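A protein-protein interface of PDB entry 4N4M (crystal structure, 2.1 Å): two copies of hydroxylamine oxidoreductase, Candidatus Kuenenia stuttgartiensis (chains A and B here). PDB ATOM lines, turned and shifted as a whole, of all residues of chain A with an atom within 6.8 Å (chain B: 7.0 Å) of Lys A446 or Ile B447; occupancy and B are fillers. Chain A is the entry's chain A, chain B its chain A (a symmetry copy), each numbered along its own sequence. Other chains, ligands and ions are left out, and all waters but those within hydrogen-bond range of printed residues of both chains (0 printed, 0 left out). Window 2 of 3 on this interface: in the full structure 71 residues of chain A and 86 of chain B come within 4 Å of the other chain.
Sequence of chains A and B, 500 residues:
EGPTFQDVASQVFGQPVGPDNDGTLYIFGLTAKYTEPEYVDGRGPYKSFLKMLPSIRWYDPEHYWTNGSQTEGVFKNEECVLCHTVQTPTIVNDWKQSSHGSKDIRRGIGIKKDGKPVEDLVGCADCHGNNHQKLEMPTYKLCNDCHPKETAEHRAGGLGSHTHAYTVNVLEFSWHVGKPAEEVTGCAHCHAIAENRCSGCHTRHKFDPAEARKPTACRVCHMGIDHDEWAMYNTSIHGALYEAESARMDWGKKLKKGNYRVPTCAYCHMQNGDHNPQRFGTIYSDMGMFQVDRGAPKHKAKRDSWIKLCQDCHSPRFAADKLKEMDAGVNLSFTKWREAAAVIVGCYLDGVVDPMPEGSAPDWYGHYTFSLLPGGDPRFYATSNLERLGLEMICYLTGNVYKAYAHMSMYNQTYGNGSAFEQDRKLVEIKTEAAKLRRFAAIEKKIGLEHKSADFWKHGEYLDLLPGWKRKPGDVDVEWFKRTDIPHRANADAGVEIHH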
ATOM      1  N   ALA A 441      -8.352  20.387  -3.051  1.00  0.00           N
ATOM      2  CA  ALA A 441      -8.833  19.037  -3.364  1.00  0.00           C
ATOM      3  C   ALA A 441      -9.111  18.858  -4.857  1.00  0.00           C
ATOM      4  O   ALA A 441      -8.796  17.813  -5.424  1.00  0.00           O
ATOM      5  CB  ALA A 441     -10.090  18.713  -2.553  1.00  0.00           C
ATOM      6  N   ALA A 442      -9.696  19.880  -5.482  1.00  0.00           N
ATOM      7  CA  ALA A 442      -9.982  19.861  -6.917  1.00  0.00           C
ATOM      8  C   ALA A 442      -8.702  19.778  -7.753  1.00  0.00           C
ATOM      9  O   ALA A 442      -8.647  19.034  -8.737  1.00  0.00           O
ATOM     10  CB  ALA A 442     -10.792  21.088  -7.315  1.00  0.00           C
ATOM     11  N   ILE A 443      -7.682  20.541  -7.360  1.00  0.00           N
ATOM     12  CA  ILE A 443      -6.388  20.514  -8.043  1.00  0.00           C
ATOM     13  C   ILE A 443      -5.712  19.152  -7.869  1.00  0.00           C
ATOM     14  O   ILE A 443      -5.335  18.514  -8.852  1.00  0.00           O
ATOM     15  CB  ILE A 443      -5.448  21.646  -7.545  1.00  0.00           C
ATOM     16  CG1 ILE A 443      -5.910  22.996  -8.101  1.00  0.00           C
ATOM     17  CG2 ILE A 443      -4.008  21.391  -7.969  1.00  0.00           C
ATOM     18  CD1 ILE A 443      -5.149  24.186  -7.550  1.00  0.00           C
ATOM     19  N   GLU A 444      -5.585  18.708  -6.622  1.00  0.00           N
ATOM     20  CA  GLU A 444      -4.954  17.420  -6.303  1.00  0.00           C
ATOM     21  C   GLU A 444      -5.607  16.230  -7.020  1.00  0.00           C
ATOM     22  O   GLU A 444      -4.915  15.313  -7.461  1.00  0.00           O
ATOM     23  CB  GLU A 444      -4.954  17.199  -4.786  1.00  0.00           C
ATOM     24  CG  GLU A 444      -3.914  18.060  -4.060  1.00  0.00           C
ATOM     25  CD  GLU A 444      -4.168  18.207  -2.565  1.00  0.00           C
ATOM     26  OE1 GLU A 444      -3.403  18.950  -1.914  1.00  0.00           O
ATOM     27  OE2 GLU A 444      -5.122  17.588  -2.040  1.00  0.00           O
ATOM     28  N   LYS A 445      -6.933  16.253  -7.122  1.00  0.00           N
ATOM     29  CA  LYS A 445      -7.695  15.258  -7.883  1.00  0.00           C
ATOM     30  C   LYS A 445      -7.247  15.252  -9.348  1.00  0.00           C
ATOM     31  O   LYS A 445      -6.830  14.218  -9.866  1.00  0.00           O
ATOM     32  CB  LYS A 445      -9.199  15.563  -7.776  1.00  0.00           C
ATOM     33  CG  LYS A 445     -10.132  14.727  -8.662  1.00  0.00           C
ATOM     34  CD  LYS A 445     -10.431  13.358  -8.068  1.00  0.00           C
ATOM     35  CE  LYS A 445     -11.333  12.541  -8.992  1.00  0.00           C
ATOM     36  NZ  LYS A 445     -12.659  13.198  -9.206  1.00  0.00           N
ATOM     37  N   LYS A 446      -7.310  16.417  -9.988  1.00  0.00           N
ATOM     38  CA  LYS A 446      -7.017  16.557 -11.418  1.00  0.00           C
ATOM     39  C   LYS A 446      -5.576  16.193 -11.793  1.00  0.00           C
ATOM     40  O   LYS A 446      -5.356  15.535 -12.809  1.00  0.00           O
ATOM     41  CB  LYS A 446      -7.326  17.981 -11.892  1.00  0.00           C
ATOM     42  CG  LYS A 446      -7.377  18.147 -13.411  1.00  0.00           C
ATOM     43  CD  LYS A 446      -7.227  19.605 -13.810  1.00  0.00           C
ATOM     44  CE  LYS A 446      -7.065  19.769 -15.315  1.00  0.00           C
ATOM     45  NZ  LYS A 446      -8.326  19.499 -16.051  1.00  0.00           N
ATOM     46  N   ILE A 447      -4.601  16.621 -10.994  1.00  0.00           N
ATOM     47  CA  ILE A 447      -3.194  16.286 -11.263  1.00  0.00           C
ATOM     48  C   ILE A 447      -2.786  14.920 -10.694  1.00  0.00           C
ATOM     49  O   ILE A 447      -1.670  14.456 -10.929  1.00  0.00           O
ATOM     50  CB  ILE A 447      -2.216  17.380 -10.752  1.00  0.00           C
ATOM     51  CG1 ILE A 447      -2.162  17.428  -9.219  1.00  0.00           C
ATOM     52  CG2 ILE A 447      -2.602  18.742 -11.318  1.00  0.00           C
ATOM     53  CD1 ILE A 447      -1.076  18.337  -8.683  1.00  0.00           C
ATOM     54  N   GLY A 448      -3.681  14.292  -9.935  1.00  0.00           N
ATOM     55  CA  GLY A 448      -3.428  12.969  -9.376  1.00  0.00           C
ATOM     56  C   GLY A 448      -2.454  12.944  -8.212  1.00  0.00           C
ATOM     57  O   GLY A 448      -1.739  11.958  -8.025  1.00  0.00           O
ATOM     58  N   LEU A 449      -2.423  14.017  -7.421  1.00  0.00           N
ATOM     59  CA  LEU A 449      -1.619  14.039  -6.196  1.00  0.00           C
ATOM     60  C   LEU A 449      -2.427  13.416  -5.061  1.00  0.00           C
ATOM     61  O   LEU A 449      -3.584  13.767  -4.842  1.00  0.00           O
ATOM     62  CB  LEU A 449      -1.193  15.466  -5.830  1.00  0.00           C
ATOM     63  CG  LEU A 449       0.083  15.597  -4.982  1.00  0.00           C
ATOM     64  CD1 LEU A 449       0.588  17.031  -4.991  1.00  0.00           C
ATOM     65  CD2 LEU A 449      -0.132  15.126  -3.551  1.00  0.00           C
ATOM     66  N   ALA B 442      -2.527  30.876 -10.463  1.00  0.00           N
ATOM     67  CA  ALA B 442      -1.364  30.494 -11.266  1.00  0.00           C
ATOM     68  C   ALA B 442      -1.336  28.990 -11.548  1.00  0.00           C
ATOM     69  O   ALA B 442      -1.035  28.572 -12.670  1.00  0.00           O
ATOM     70  CB  ALA B 442      -0.077  30.925 -10.577  1.00  0.00           C
ATOM     71  N   ILE B 443      -1.648  28.185 -10.531  1.00  0.00           N
ATOM     72  CA  ILE B 443      -1.708  26.731 -10.685  1.00  0.00           C
ATOM     73  C   ILE B 443      -2.847  26.333 -11.626  1.00  0.00           C
ATOM     74  O   ILE B 443      -2.625  25.618 -12.604  1.00  0.00           O
ATOM     75  CB  ILE B 443      -1.865  26.011  -9.318  1.00  0.00           C
ATOM     76  CG1 ILE B 443      -0.541  26.051  -8.547  1.00  0.00           C
ATOM     77  CG2 ILE B 443      -2.297  24.564  -9.506  1.00  0.00           C
ATOM     78  CD1 ILE B 443      -0.632  25.508  -7.134  1.00  0.00           C
ATOM     79  N   GLU B 444      -4.052  26.816 -11.336  1.00  0.00           N
ATOM     80  CA  GLU B 444      -5.238  26.515 -12.148  1.00  0.00           C
ATOM     81  C   GLU B 444      -5.073  26.887 -13.628  1.00  0.00           C
ATOM     82  O   GLU B 444      -5.531  26.159 -14.508  1.00  0.00           O
ATOM     83  CB  GLU B 444      -6.469  27.211 -11.553  1.00  0.00           C
ATOM     84  CG  GLU B 444      -6.980  26.528 -10.279  1.00  0.00           C
ATOM     85  CD  GLU B 444      -7.890  27.407  -9.431  1.00  0.00           C
ATOM     86  OE1 GLU B 444      -8.294  26.947  -8.341  1.00  0.00           O
ATOM     87  OE2 GLU B 444      -8.202  28.547  -9.843  1.00  0.00           O
ATOM     88  N   LYS B 445      -4.426  28.021 -13.886  1.00  0.00           N
ATOM     89  CA  LYS B 445      -4.078  28.452 -15.243  1.00  0.00           C
ATOM     90  C   LYS B 445      -3.197  27.402 -15.926  1.00  0.00           C
ATOM     91  O   LYS B 445      -3.544  26.895 -16.991  1.00  0.00           O
ATOM     92  CB  LYS B 445      -3.359  29.812 -15.188  1.00  0.00           C
ATOM     93  CG  LYS B 445      -2.762  30.325 -16.504  1.00  0.00           C
ATOM     94  CD  LYS B 445      -3.802  30.982 -17.400  1.00  0.00           C
ATOM     95  CE  LYS B 445      -3.180  31.450 -18.715  1.00  0.00           C
ATOM     96  NZ  LYS B 445      -2.113  32.475 -18.498  1.00  0.00           N
ATOM     97  N   LYS B 446      -2.079  27.065 -15.286  1.00  0.00           N
ATOM     98  CA  LYS B 446      -1.080  26.154 -15.854  1.00  0.00           C
ATOM     99  C   LYS B 446      -1.607  24.738 -16.108  1.00  0.00           C
ATOM    100  O   LYS B 446      -1.306  24.150 -17.147  1.00  0.00           O
ATOM    101  CB  LYS B 446       0.158  26.087 -14.953  1.00  0.00           C
ATOM    102  CG  LYS B 446       1.382  25.441 -15.604  1.00  0.00           C
ATOM    103  CD  LYS B 446       2.389  24.994 -14.557  1.00  0.00           C
ATOM    104  CE  LYS B 446       3.511  24.165 -15.166  1.00  0.00           C
ATOM    105  NZ  LYS B 446       4.438  24.985 -15.986  1.00  0.00           N
ATOM    106  N   ILE B 447      -2.376  24.186 -15.172  1.00  0.00           N
ATOM    107  CA  ILE B 447      -2.950  22.843 -15.352  1.00  0.00           C
ATOM    108  C   ILE B 447      -4.268  22.860 -16.139  1.00  0.00           C
ATOM    109  O   ILE B 447      -4.815  21.804 -16.460  1.00  0.00           O
ATOM    110  CB  ILE B 447      -3.153  22.099 -14.004  1.00  0.00           C
ATOM    111  CG1 ILE B 447      -4.275  22.729 -13.167  1.00  0.00           C
ATOM    112  CG2 ILE B 447      -1.849  22.065 -13.216  1.00  0.00           C
ATOM    113  CD1 ILE B 447      -4.640  21.917 -11.942  1.00  0.00           C
ATOM    114  N   GLY B 448      -4.782  24.053 -16.429  1.00  0.00           N
ATOM    115  CA  GLY B 448      -6.005  24.199 -17.211  1.00  0.00           C
ATOM    116  C   GLY B 448      -7.282  23.852 -16.467  1.00  0.00           C
ATOM    117  O   GLY B 448      -8.247  23.390 -17.078  1.00  0.00           O
ATOM    118  N   LEU B 449      -7.303  24.078 -15.153  1.00  0.00           N
ATOM    119  CA  LEU B 449      -8.528  23.905 -14.368  1.00  0.00           C
ATOM    120  C   LEU B 449      -9.352  25.187 -14.446  1.00  0.00           C
ATOM    121  O   LEU B 449      -8.837  26.283 -14.234  1.00  0.00           O
ATOM    122  CB  LEU B 449      -8.215  23.556 -12.908  1.00  0.00           C
ATOM    123  CG  LEU B 449      -9.304  22.786 -12.145  1.00  0.00           C
ATOM    124  CD1 LEU B 449      -8.746  22.199 -10.858  1.00  0.00           C
ATOM    125  CD2 LEU B 449     -10.514  23.658 -11.842  1.00  0.00           C
ATOM    126  N   GLU B 450     -10.633  25.030 -14.759  1.00  0.00           N
ATOM    127  CA  GLU B 450     -11.574  26.144 -14.831  1.00  0.00           C
ATOM    128  C   GLU B 450     -12.270  26.266 -13.471  1.00  0.00           C
ATOM    129  O   GLU B 450     -13.211  25.531 -13.168  1.00  0.00           O
ATOM    130  CB  GLU B 450     -12.589  25.942 -15.977  1.00  0.00           C
ATOM    131  CG  GLU B 450     -13.444  24.645 -15.941  1.00  0.00           C
ATOM    132  CD  GLU B 450     -12.692  23.391 -16.396  1.00  0.00           C
ATOM    133  OE1 GLU B 450     -12.373  22.533 -15.535  1.00  0.00           O
ATOM    134  OE2 GLU B 450     -12.418  23.269 -17.614  1.00  0.00           O
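Of the 9 printed residues of chain B, 3 touch a printed residue of chain A.
Hydrophobic or aromatic side chains of chain B within 4 Å of the printed part of chain A: Ile B443, Ile B447 and Leu B449.
Along chain B the printed residues that touch a printed residue of chain A span positions 443 to 449.
Among the printed residues, no Asp or Glu carboxylate lies within 4 Å of a Lys or Arg side-chain nitrogen of the other chain.
Ala A442 touches Leu B449, but with the chains exchanged Leu A449 does not touch Ala B442 (13.8 Å).
Ile B443 touches its own counterpart, Ile A443.
Lys A446 touches Ile B447, but with the chains exchanged Ile A447 does not touch Lys B446 (7.7 Å).
Ile A447 touches its own counterpart, Ile B447.
Positions printed for both chains: 442, 443, 444, 445, 446, 447, 448 and 449.
Of the printed residues of chain B, Lys A446 touches Ile B447.
Of the printed residues of chain B, Ile A447 touches Ile B447 (3.8 Å).
Gly A448 touches none of the printed residues of chain B.
Leu A449 touches none of the printed residues of chain B.
Printed residues of chain A within 4 Å of Ile B443: Ile A443.
Ile B447 touches two residues of chain A.
Of the printed residues of chain A, Leu B449 touches Ala A442.
The nearest printed residue of chain B that does not touch Ile A443 is Leu B449 (4.01 Å).
N of Leu B449 is in hydrogen-bond range of O of Glu B444 (2.8 Å).
Leu B449 touches Ala A442 (CD1 to O, 3.8 Å).
Ile B443 touches Ile A443.
Lys A446 touches Ile B447 (CE to O, 3.2 Å).
CD1 of Ile B447 touches CG2 of Ile A447, 3.8 Å away.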
